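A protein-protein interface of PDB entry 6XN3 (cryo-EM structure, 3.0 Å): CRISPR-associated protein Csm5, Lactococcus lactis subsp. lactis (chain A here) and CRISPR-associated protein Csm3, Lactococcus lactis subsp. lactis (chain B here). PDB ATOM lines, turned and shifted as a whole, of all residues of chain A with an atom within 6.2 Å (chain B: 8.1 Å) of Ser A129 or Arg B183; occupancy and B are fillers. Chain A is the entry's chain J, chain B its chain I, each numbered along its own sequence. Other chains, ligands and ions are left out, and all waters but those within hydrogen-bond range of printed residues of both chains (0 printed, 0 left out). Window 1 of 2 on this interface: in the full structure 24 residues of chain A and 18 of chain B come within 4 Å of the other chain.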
ATOM      1  N   PRO A 127      29.092  10.040  15.228  1.00  0.00           N
ATOM      2  CA  PRO A 127      27.702   9.593  15.309  1.00  0.00           C
ATOM      3  C   PRO A 127      27.430   8.868  16.617  1.00  0.00           C
ATOM      4  O   PRO A 127      28.335   8.315  17.243  1.00  0.00           O
ATOM      5  CB  PRO A 127      27.565   8.655  14.109  1.00  0.00           C
ATOM      6  CG  PRO A 127      28.925   8.191  13.846  1.00  0.00           C
ATOM      7  CD  PRO A 127      29.848   9.303  14.209  1.00  0.00           C
ATOM      8  N   GLY A 128      26.160   8.882  17.028  1.00  0.00           N
ATOM      9  CA  GLY A 128      25.781   8.313  18.311  1.00  0.00           C
ATOM     10  C   GLY A 128      25.840   6.804  18.361  1.00  0.00           C
ATOM     11  O   GLY A 128      25.930   6.232  19.456  1.00  0.00           O
ATOM     12  N   SER A 129      25.792   6.144  17.202  1.00  0.00           N
ATOM     13  CA  SER A 129      25.923   4.694  17.166  1.00  0.00           C
ATOM     14  C   SER A 129      27.309   4.259  17.614  1.00  0.00           C
ATOM     15  O   SER A 129      27.461   3.209  18.250  1.00  0.00           O
ATOM     16  CB  SER A 129      25.634   4.177  15.761  1.00  0.00           C
ATOM     17  OG  SER A 129      26.807   4.199  14.969  1.00  0.00           O
ATOM     18  N   SER A 130      28.326   5.072  17.312  1.00  0.00           N
ATOM     19  CA  SER A 130      29.686   4.799  17.762  1.00  0.00           C
ATOM     20  C   SER A 130      29.771   4.805  19.279  1.00  0.00           C
ATOM     21  O   SER A 130      30.348   3.895  19.891  1.00  0.00           O
ATOM     22  CB  SER A 130      30.635   5.846  17.194  1.00  0.00           C
ATOM     23  OG  SER A 130      30.660   5.798  15.789  1.00  0.00           O
ATOM     24  N   LEU A 131      29.174   5.819  19.904  1.00  0.00           N
ATOM     25  CA  LEU A 131      29.257   5.930  21.350  1.00  0.00           C
ATOM     26  C   LEU A 131      28.422   4.852  22.021  1.00  0.00           C
ATOM     27  O   LEU A 131      28.812   4.326  23.069  1.00  0.00           O
ATOM     28  CB  LEU A 131      28.815   7.317  21.798  1.00  0.00           C
ATOM     29  CG  LEU A 131      29.051   7.577  23.282  1.00  0.00           C
ATOM     30  CD1 LEU A 131      30.530   7.477  23.550  1.00  0.00           C
ATOM     31  CD2 LEU A 131      28.516   8.906  23.730  1.00  0.00           C
ATOM     32  N   LYS A 132      27.285   4.486  21.419  1.00  0.00           N
ATOM     33  CA  LYS A 132      26.502   3.394  21.988  1.00  0.00           C
ATOM     34  C   LYS A 132      27.234   2.066  21.865  1.00  0.00           C
ATOM     35  O   LYS A 132      27.167   1.239  22.776  1.00  0.00           O
ATOM     36  CB  LYS A 132      25.119   3.304  21.346  1.00  0.00           C
ATOM     37  CG  LYS A 132      24.266   2.244  22.015  1.00  0.00           C
ATOM     38  CD  LYS A 132      22.887   2.100  21.483  1.00  0.00           C
ATOM     39  CE  LYS A 132      22.007   3.092  22.154  1.00  0.00           C
ATOM     40  NZ  LYS A 132      20.585   2.762  21.953  1.00  0.00           N
ATOM     41  N   GLY A 133      27.971   1.861  20.773  1.00  0.00           N
ATOM     42  CA  GLY A 133      28.784   0.661  20.666  1.00  0.00           C
ATOM     43  C   GLY A 133      29.886   0.609  21.706  1.00  0.00           C
ATOM     44  O   GLY A 133      30.156  -0.448  22.286  1.00  0.00           O
ATOM     45  N   ALA A 134      30.501   1.760  21.985  1.00  0.00           N
ATOM     46  CA  ALA A 134      31.519   1.823  23.029  1.00  0.00           C
ATOM     47  C   ALA A 134      30.938   1.529  24.406  1.00  0.00           C
ATOM     48  O   ALA A 134      31.484   0.708  25.152  1.00  0.00           O
ATOM     49  CB  ALA A 134      32.184   3.189  23.026  1.00  0.00           C
ATOM     50  N   LEU A 156      18.498   3.227  26.220  1.00  0.00           N
ATOM     51  CA  LEU A 156      19.648   4.123  26.310  1.00  0.00           C
ATOM     52  C   LEU A 156      19.574   5.034  25.091  1.00  0.00           C
ATOM     53  O   LEU A 156      19.696   4.570  23.956  1.00  0.00           O
ATOM     54  CB  LEU A 156      20.952   3.338  26.375  1.00  0.00           C
ATOM     55  CG  LEU A 156      22.278   4.035  26.685  1.00  0.00           C
ATOM     56  CD1 LEU A 156      23.184   3.034  27.353  1.00  0.00           C
ATOM     57  CD2 LEU A 156      22.969   4.560  25.450  1.00  0.00           C
ATOM     58  N   GLN A 157      19.381   6.326  25.328  1.00  0.00           N
ATOM     59  CA  GLN A 157      19.129   7.303  24.277  1.00  0.00           C
ATOM     60  C   GLN A 157      20.362   8.175  24.099  1.00  0.00           C
ATOM     61  O   GLN A 157      20.528   9.158  24.823  1.00  0.00           O
ATOM     62  CB  GLN A 157      17.945   8.185  24.660  1.00  0.00           C
ATOM     63  CG  GLN A 157      16.623   7.487  24.767  1.00  0.00           C
ATOM     64  CD  GLN A 157      16.190   6.903  23.466  1.00  0.00           C
ATOM     65  OE1 GLN A 157      16.175   5.689  23.281  1.00  0.00           O
ATOM     66  NE2 GLN A 157      15.860   7.773  22.531  1.00  0.00           N
ATOM     67  N   VAL A 158      21.209   7.845  23.131  1.00  0.00           N
ATOM     68  CA  VAL A 158      22.419   8.616  22.878  1.00  0.00           C
ATOM     69  C   VAL A 158      22.308   9.302  21.521  1.00  0.00           C
ATOM     70  O   VAL A 158      21.933   8.679  20.523  1.00  0.00           O
ATOM     71  CB  VAL A 158      23.691   7.747  23.001  1.00  0.00           C
ATOM     72  CG1 VAL A 158      23.613   6.526  22.148  1.00  0.00           C
ATOM     73  CG2 VAL A 158      24.918   8.534  22.605  1.00  0.00           C
ATOM     74  N   SER A 159      22.559  10.605  21.505  1.00  0.00           N
ATOM     75  CA  SER A 159      22.517  11.401  20.292  1.00  0.00           C
ATOM     76  C   SER A 159      23.909  11.542  19.704  1.00  0.00           C
ATOM     77  O   SER A 159      24.880  10.959  20.185  1.00  0.00           O
ATOM     78  CB  SER A 159      21.933  12.783  20.572  1.00  0.00           C
ATOM     79  OG  SER A 159      22.031  13.604  19.425  1.00  0.00           O
ATOM     80  N   ASP A 160      23.995  12.331  18.646  1.00  0.00           N
ATOM     81  CA  ASP A 160      25.282  12.668  18.073  1.00  0.00           C
ATOM     82  C   ASP A 160      25.894  13.844  18.815  1.00  0.00           C
ATOM     83  O   ASP A 160      25.360  14.332  19.811  1.00  0.00           O
ATOM     84  CB  ASP A 160      25.150  13.001  16.592  1.00  0.00           C
ATOM     85  CG  ASP A 160      24.671  11.831  15.786  1.00  0.00           C
ATOM     86  OD1 ASP A 160      24.654  10.713  16.332  1.00  0.00           O
ATOM     87  OD2 ASP A 160      24.320  12.020  14.606  1.00  0.00           O
ATOM     88  N   THR B  13      19.366  16.433  13.714  1.00  0.00           N
ATOM     89  CA  THR B  13      20.151  15.224  13.507  1.00  0.00           C
ATOM     90  C   THR B  13      19.540  14.568  12.256  1.00  0.00           C
ATOM     91  O   THR B  13      18.814  15.221  11.506  1.00  0.00           O
ATOM     92  CB  THR B  13      20.142  14.411  14.820  1.00  0.00           C
ATOM     93  OG1 THR B  13      20.560  15.261  15.888  1.00  0.00           O
ATOM     94  CG2 THR B  13      21.213  13.325  14.855  1.00  0.00           C
ATOM     95  N   LYS B 118      24.632   7.235   5.528  1.00  0.00           N
ATOM     96  CA  LYS B 118      25.417   7.091   6.742  1.00  0.00           C
ATOM     97  C   LYS B 118      25.907   5.659   6.880  1.00  0.00           C
ATOM     98  O   LYS B 118      25.136   4.710   6.731  1.00  0.00           O
ATOM     99  CB  LYS B 118      24.581   7.480   7.956  1.00  0.00           C
ATOM    100  CG  LYS B 118      25.295   7.364   9.273  1.00  0.00           C
ATOM    101  CD  LYS B 118      24.290   7.331  10.399  1.00  0.00           C
ATOM    102  CE  LYS B 118      24.964   7.449  11.745  1.00  0.00           C
ATOM    103  NZ  LYS B 118      24.319   6.571  12.757  1.00  0.00           N
ATOM    104  N   PHE B 119      27.193   5.506   7.168  1.00  0.00           N
ATOM    105  CA  PHE B 119      27.820   4.197   7.223  1.00  0.00           C
ATOM    106  C   PHE B 119      27.842   3.675   8.649  1.00  0.00           C
ATOM    107  O   PHE B 119      28.350   4.335   9.557  1.00  0.00           O
ATOM    108  CB  PHE B 119      29.240   4.258   6.676  1.00  0.00           C
ATOM    109  CG  PHE B 119      29.325   3.997   5.211  1.00  0.00           C
ATOM    110  CD1 PHE B 119      28.806   4.904   4.306  1.00  0.00           C
ATOM    111  CD2 PHE B 119      29.909   2.840   4.734  1.00  0.00           C
ATOM    112  CE1 PHE B 119      28.878   4.670   2.950  1.00  0.00           C
ATOM    113  CE2 PHE B 119      29.984   2.598   3.381  1.00  0.00           C
ATOM    114  CZ  PHE B 119      29.466   3.516   2.487  1.00  0.00           C
ATOM    115  N   GLU B 120      27.290   2.479   8.835  1.00  0.00           N
ATOM    116  CA  GLU B 120      27.258   1.814  10.128  1.00  0.00           C
ATOM    117  C   GLU B 120      27.725   0.380   9.930  1.00  0.00           C
ATOM    118  O   GLU B 120      27.868  -0.084   8.798  1.00  0.00           O
ATOM    119  CB  GLU B 120      25.858   1.862  10.754  1.00  0.00           C
ATOM    120  CG  GLU B 120      25.518   3.202  11.394  1.00  0.00           C
ATOM    121  CD  GLU B 120      24.154   3.225  12.072  1.00  0.00           C
ATOM    122  OE1 GLU B 120      23.575   4.325  12.207  1.00  0.00           O
ATOM    123  OE2 GLU B 120      23.659   2.155  12.471  1.00  0.00           O
ATOM    124  N   ASN B 121      27.991  -0.313  11.036  1.00  0.00           N
ATOM    125  CA  ASN B 121      28.234  -1.748  10.975  1.00  0.00           C
ATOM    126  C   ASN B 121      27.791  -2.374  12.287  1.00  0.00           C
ATOM    127  O   ASN B 121      27.170  -1.727  13.131  1.00  0.00           O
ATOM    128  CB  ASN B 121      29.695  -2.094  10.600  1.00  0.00           C
ATOM    129  CG  ASN B 121      30.760  -1.694  11.636  1.00  0.00           C
ATOM    130  OD1 ASN B 121      30.500  -1.377  12.788  1.00  0.00           O
ATOM    131  ND2 ASN B 121      32.004  -1.704  11.178  1.00  0.00           N
ATOM    132  N   THR B 122      28.122  -3.647  12.447  1.00  0.00           N
ATOM    133  CA  THR B 122      27.919  -4.363  13.692  1.00  0.00           C
ATOM    134  C   THR B 122      29.111  -5.269  13.919  1.00  0.00           C
ATOM    135  O   THR B 122      29.407  -6.124  13.082  1.00  0.00           O
ATOM    136  CB  THR B 122      26.640  -5.189  13.662  1.00  0.00           C
ATOM    137  OG1 THR B 122      25.550  -4.356  13.254  1.00  0.00           O
ATOM    138  CG2 THR B 122      26.352  -5.760  15.032  1.00  0.00           C
ATOM    139  N   ARG B 125      30.944  -9.552  18.790  1.00  0.00           N
ATOM    140  CA  ARG B 125      31.971  -9.408  19.810  1.00  0.00           C
ATOM    141  C   ARG B 125      32.760 -10.685  20.059  1.00  0.00           C
ATOM    142  O   ARG B 125      33.728 -10.652  20.825  1.00  0.00           O
ATOM    143  CB  ARG B 125      31.341  -8.926  21.110  1.00  0.00           C
ATOM    144  CG  ARG B 125      31.252  -7.430  21.258  1.00  0.00           C
ATOM    145  CD  ARG B 125      29.970  -6.882  20.680  1.00  0.00           C
ATOM    146  NE  ARG B 125      29.943  -5.428  20.752  1.00  0.00           N
ATOM    147  CZ  ARG B 125      29.551  -4.744  21.819  1.00  0.00           C
ATOM    148  NH1 ARG B 125      29.148  -5.384  22.908  1.00  0.00           N
ATOM    149  NH2 ARG B 125      29.568  -3.421  21.801  1.00  0.00           N
ATOM    150  N   ARG B 133      26.437  -1.771   6.995  1.00  0.00           N
ATOM    151  CA  ARG B 133      25.167  -1.342   6.436  1.00  0.00           C
ATOM    152  C   ARG B 133      25.269   0.131   6.082  1.00  0.00           C
ATOM    153  O   ARG B 133      26.113   0.847   6.618  1.00  0.00           O
ATOM    154  CB  ARG B 133      24.018  -1.555   7.415  1.00  0.00           C
ATOM    155  CG  ARG B 133      24.308  -1.026   8.786  1.00  0.00           C
ATOM    156  CD  ARG B 133      23.064  -1.040   9.636  1.00  0.00           C
ATOM    157  NE  ARG B 133      23.246  -0.351  10.904  1.00  0.00           N
ATOM    158  CZ  ARG B 133      23.821  -0.895  11.971  1.00  0.00           C
ATOM    159  NH1 ARG B 133      24.283  -2.135  11.926  1.00  0.00           N
ATOM    160  NH2 ARG B 133      23.937  -0.192  13.086  1.00  0.00           N
ATOM    161  N   ILE B 135      22.529   3.503   5.616  1.00  0.00           N
ATOM    162  CA  ILE B 135      21.170   4.001   5.783  1.00  0.00           C
ATOM    163  C   ILE B 135      21.073   5.384   5.156  1.00  0.00           C
ATOM    164  O   ILE B 135      22.006   6.187   5.256  1.00  0.00           O
ATOM    165  CB  ILE B 135      20.733   4.016   7.261  1.00  0.00           C
ATOM    166  CG1 ILE B 135      21.726   4.780   8.128  1.00  0.00           C
ATOM    167  CG2 ILE B 135      20.559   2.607   7.778  1.00  0.00           C
ATOM    168  CD1 ILE B 135      21.251   5.002   9.529  1.00  0.00           C
ATOM    169  N   ARG B 137      19.784   8.948   5.164  1.00  0.00           N
ATOM    170  CA  ARG B 137      19.424   9.760   6.308  1.00  0.00           C
ATOM    171  C   ARG B 137      19.345  11.202   5.843  1.00  0.00           C
ATOM    172  O   ARG B 137      20.241  11.669   5.136  1.00  0.00           O
ATOM    173  CB  ARG B 137      20.464   9.572   7.413  1.00  0.00           C
ATOM    174  CG  ARG B 137      19.920   9.556   8.806  1.00  0.00           C
ATOM    175  CD  ARG B 137      21.055   9.443   9.794  1.00  0.00           C
ATOM    176  NE  ARG B 137      21.937  10.596   9.686  1.00  0.00           N
ATOM    177  CZ  ARG B 137      22.845  10.929  10.590  1.00  0.00           C
ATOM    178  NH1 ARG B 137      22.980  10.206  11.689  1.00  0.00           N
ATOM    179  NH2 ARG B 137      23.606  11.996  10.403  1.00  0.00           N
ATOM    180  N   TYR B 176      13.330  10.976  19.876  1.00  0.00           N
ATOM    181  CA  TYR B 176      13.569  10.978  18.442  1.00  0.00           C
ATOM    182  C   TYR B 176      12.255  11.091  17.677  1.00  0.00           C
ATOM    183  O   TYR B 176      11.175  11.165  18.263  1.00  0.00           O
ATOM    184  CB  TYR B 176      14.328   9.720  18.028  1.00  0.00           C
ATOM    185  CG  TYR B 176      13.830   8.423  18.615  1.00  0.00           C
ATOM    186  CD1 TYR B 176      12.707   7.798  18.103  1.00  0.00           C
ATOM    187  CD2 TYR B 176      14.554   7.755  19.576  1.00  0.00           C
ATOM    188  CE1 TYR B 176      12.280   6.592  18.596  1.00  0.00           C
ATOM    189  CE2 TYR B 176      14.133   6.552  20.082  1.00  0.00           C
ATOM    190  CZ  TYR B 176      12.996   5.974  19.588  1.00  0.00           C
ATOM    191  OH  TYR B 176      12.575   4.766  20.089  1.00  0.00           O
ATOM    192  N   GLY B 179      13.050   5.905  13.291  1.00  0.00           N
ATOM    193  CA  GLY B 179      14.201   5.168  12.822  1.00  0.00           C
ATOM    194  C   GLY B 179      15.192   4.926  13.938  1.00  0.00           C
ATOM    195  O   GLY B 179      14.829   4.904  15.120  1.00  0.00           O
ATOM    196  N   HIS B 180      16.460   4.805  13.558  1.00  0.00           N
ATOM    197  CA  HIS B 180      17.532   4.500  14.500  1.00  0.00           C
ATOM    198  C   HIS B 180      17.844   5.721  15.363  1.00  0.00           C
ATOM    199  O   HIS B 180      18.910   6.324  15.280  1.00  0.00           O
ATOM    200  CB  HIS B 180      18.767   4.052  13.737  1.00  0.00           C
ATOM    201  CG  HIS B 180      18.463   3.186  12.559  1.00  0.00           C
ATOM    202  ND1 HIS B 180      17.907   1.934  12.679  1.00  0.00           N
ATOM    203  CD2 HIS B 180      18.611   3.406  11.233  1.00  0.00           C
ATOM    204  CE1 HIS B 180      17.744   1.410  11.478  1.00  0.00           C
ATOM    205  NE2 HIS B 180      18.164   2.283  10.583  1.00  0.00           N
ATOM    206  N   GLY B 181      16.885   6.072  16.220  1.00  0.00           N
ATOM    207  CA  GLY B 181      16.982   7.312  16.955  1.00  0.00           C
ATOM    208  C   GLY B 181      17.568   7.165  18.329  1.00  0.00           C
ATOM    209  O   GLY B 181      17.996   8.158  18.923  1.00  0.00           O
ATOM    210  N   THR B 182      17.594   5.947  18.853  1.00  0.00           N
ATOM    211  CA  THR B 182      18.313   5.695  20.089  1.00  0.00           C
ATOM    212  C   THR B 182      19.818   5.710  19.885  1.00  0.00           C
ATOM    213  O   THR B 182      20.565   5.756  20.864  1.00  0.00           O
ATOM    214  CB  THR B 182      17.857   4.365  20.673  1.00  0.00           C
ATOM    215  OG1 THR B 182      18.488   4.151  21.940  1.00  0.00           O
ATOM    216  CG2 THR B 182      18.153   3.238  19.723  1.00  0.00           C
ATOM    217  N   ARG B 183      20.269   5.704  18.637  1.00  0.00           N
ATOM    218  CA  ARG B 183      21.670   5.707  18.263  1.00  0.00           C
ATOM    219  C   ARG B 183      22.072   7.005  17.580  1.00  0.00           C
ATOM    220  O   ARG B 183      23.033   7.022  16.807  1.00  0.00           O
ATOM    221  CB  ARG B 183      21.926   4.514  17.353  1.00  0.00           C
ATOM    222  CG  ARG B 183      21.658   3.198  18.030  1.00  0.00           C
ATOM    223  CD  ARG B 183      22.205   2.057  17.192  1.00  0.00           C
ATOM    224  NE  ARG B 183      21.262   1.535  16.188  1.00  0.00           N
ATOM    225  CZ  ARG B 183      19.992   1.146  16.356  1.00  0.00           C
ATOM    226  NH1 ARG B 183      19.410   1.016  17.540  1.00  0.00           N
ATOM    227  NH2 ARG B 183      19.308   0.762  15.293  1.00  0.00           N
ATOM    228  N   GLY B 184      21.357   8.092  17.847  1.00  0.00           N
ATOM    229  CA  GLY B 184      21.716   9.378  17.289  1.00  0.00           C
ATOM    230  C   GLY B 184      21.017   9.774  16.007  1.00  0.00           C
ATOM    231  O   GLY B 184      21.680  10.044  15.005  1.00  0.00           O
ATOM    232  N   SER B 185      19.688   9.799  16.009  1.00  0.00           N
ATOM    233  CA  SER B 185      18.940  10.314  14.874  1.00  0.00           C
ATOM    234  C   SER B 185      17.604  10.852  15.358  1.00  0.00           C
ATOM    235  O   SER B 185      17.185  10.606  16.489  1.00  0.00           O
ATOM    236  CB  SER B 185      18.718   9.248  13.802  1.00  0.00           C
ATOM    237  OG  SER B 185      19.938   8.876  13.193  1.00  0.00           O
ATOM    238  N   GLY B 186      16.944  11.606  14.486  1.00  0.00           N
ATOM    239  CA  GLY B 186      15.577  12.008  14.729  1.00  0.00           C
ATOM    240  C   GLY B 186      15.382  13.141  15.704  1.00  0.00           C
ATOM    241  O   GLY B 186      14.276  13.292  16.232  1.00  0.00           O
ATOM    242  N   ARG B 187      16.403  13.946  15.963  1.00  0.00           N
ATOM    243  CA  ARG B 187      16.224  15.068  16.872  1.00  0.00           C
ATOM    244  C   ARG B 187      15.612  16.250  16.134  1.00  0.00           C
ATOM    245  O   ARG B 187      16.216  16.817  15.221  1.00  0.00           O
ATOM    246  CB  ARG B 187      17.555  15.458  17.506  1.00  0.00           C
ATOM    247  CG  ARG B 187      18.284  14.303  18.163  1.00  0.00           C
ATOM    248  CD  ARG B 187      17.377  13.575  19.135  1.00  0.00           C
ATOM    249  NE  ARG B 187      18.119  12.753  20.078  1.00  0.00           N
ATOM    250  CZ  ARG B 187      18.479  11.502  19.840  1.00  0.00           C
ATOM    251  NH1 ARG B 187      18.169  10.935  18.690  1.00  0.00           N
ATOM    252  NH2 ARG B 187      19.147  10.821  20.750  1.00  0.00           N
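Printed residues of chain B within 4 Å of Ser A129: Glu B120 and Arg B183. Of chain A, only Gly A128 (3.2 Å), Ser A129 (2.9 Å), Lys A132 (3.8 Å) and Val A158 (3.4 Å) come within 4 Å of Arg B183. Gly A128 touches just one residue of chain B: Arg B183. Printed residues of chain A within 4 Å of Arg B187: Val A158 (3.5 Å) and Ser A159 (3.4 Å). Printed residues of chain A within 4 Å of Thr B182: Lys A132, Leu A156, Gln A157 and Val A158. Printed residues of chain A within 4 Å of Lys B118: Pro A127 (3.7 Å). The nearest residue of chain B that does not touch Ser A129 is Lys B118 (4.1 Å). The nearest residue of chain A that does not touch Arg B183 is Asp A160 (4.1 Å). The nearest printed residue of chain A that does not touch Glu B120 is Pro A127 (6.2 Å).
The side-chain hydroxyl (OG1) of Thr B182 is in hydrogen-bond range of the side-chain amino group (NZ) of Lys A132 (2.5 Å). The backbone carbonyl oxygen (O) of Thr B182 is in hydrogen-bond range of the backbone NH (N) of Val A158, at 3.1 Å. The side-chain hydroxyl (OG1) of Thr B182 sits at hydrogen-bond distance from the side-chain amide oxygen (OE1) of Gln A157, at 3.1 Å. The backbone NH (N) of Gly B184 lies within hydrogen-bond range of the backbone carbonyl oxygen (O) of Val A158. The backbone carbonyl oxygen (O) of Arg B183 lies within hydrogen-bond range of the backbone NH (N) of Ser A129 (2.9 Å). The backbone carbonyl oxygen of Leu A156 sits close to the side-chain hydroxyl of Thr B182, 2.4 Å away. The backbone carbonyl oxygen (O) of Gly B184 sits close to the side-chain carboxylate (OD2) of Asp A160, at 3.3 Å. NH1 of Arg B137 lies within salt-bridge range of OD2 of Asp A160, 3.7 Å away. NH2 of Arg B125 is in hydrogen-bond range of O of Gly A133 (3.1 Å).
The backbone carbonyl oxygen (O) of Ile B135 is in hydrogen-bond range of the backbone NH (N) of Lys B118. OD1 of Asp A160 is in hydrogen-bond range of N of Gly A128, 2.5 Å away. The side-chain amino group of Lys B118 is in salt-bridge range of the side-chain carboxylate of Glu B120, 2.4 Å away. The backbone carbonyl oxygen (O) of Gly B181 sits at hydrogen-bond distance from the guanidinium group (NH1) of Arg B187 (2.8 Å). The backbone carbonyl oxygen (O) of Ser B185 is in hydrogen-bond range of the guanidinium group (NH1) of Arg B187 (2.4 Å). The backbone carbonyl oxygen of Leu A156 lies within hydrogen-bond range of the side-chain amino group of Lys A132 (2.8 Å).
Hydrophobic or aromatic side chains of chain B that line the printed part of chain A: Tyr B176. Printed residues of chain A that touch a printed residue of chain B: Pro A127, Gly A128, Ser A129, Lys A132, Gly A133, Leu A156, Gln A157, Val A158, Ser A159 and Asp A160. Hydrophobic or aromatic side chains of chain A within 4 Å of the printed part of chain B: Pro A127 and Val A158.
Among the printed residues, merely in contact across the chains: Pro A127 with Lys B118, Gly A128 with Arg B183, Ser A129 with Glu B120, Lys A132 with Arg B183, Gln A157 with Tyr B176, Val A158 with Arg B183, Val A158 with Arg B187, Ser A159 with Gly B184, Ser A159 with Arg B187 and Asp A160 with Thr B13.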
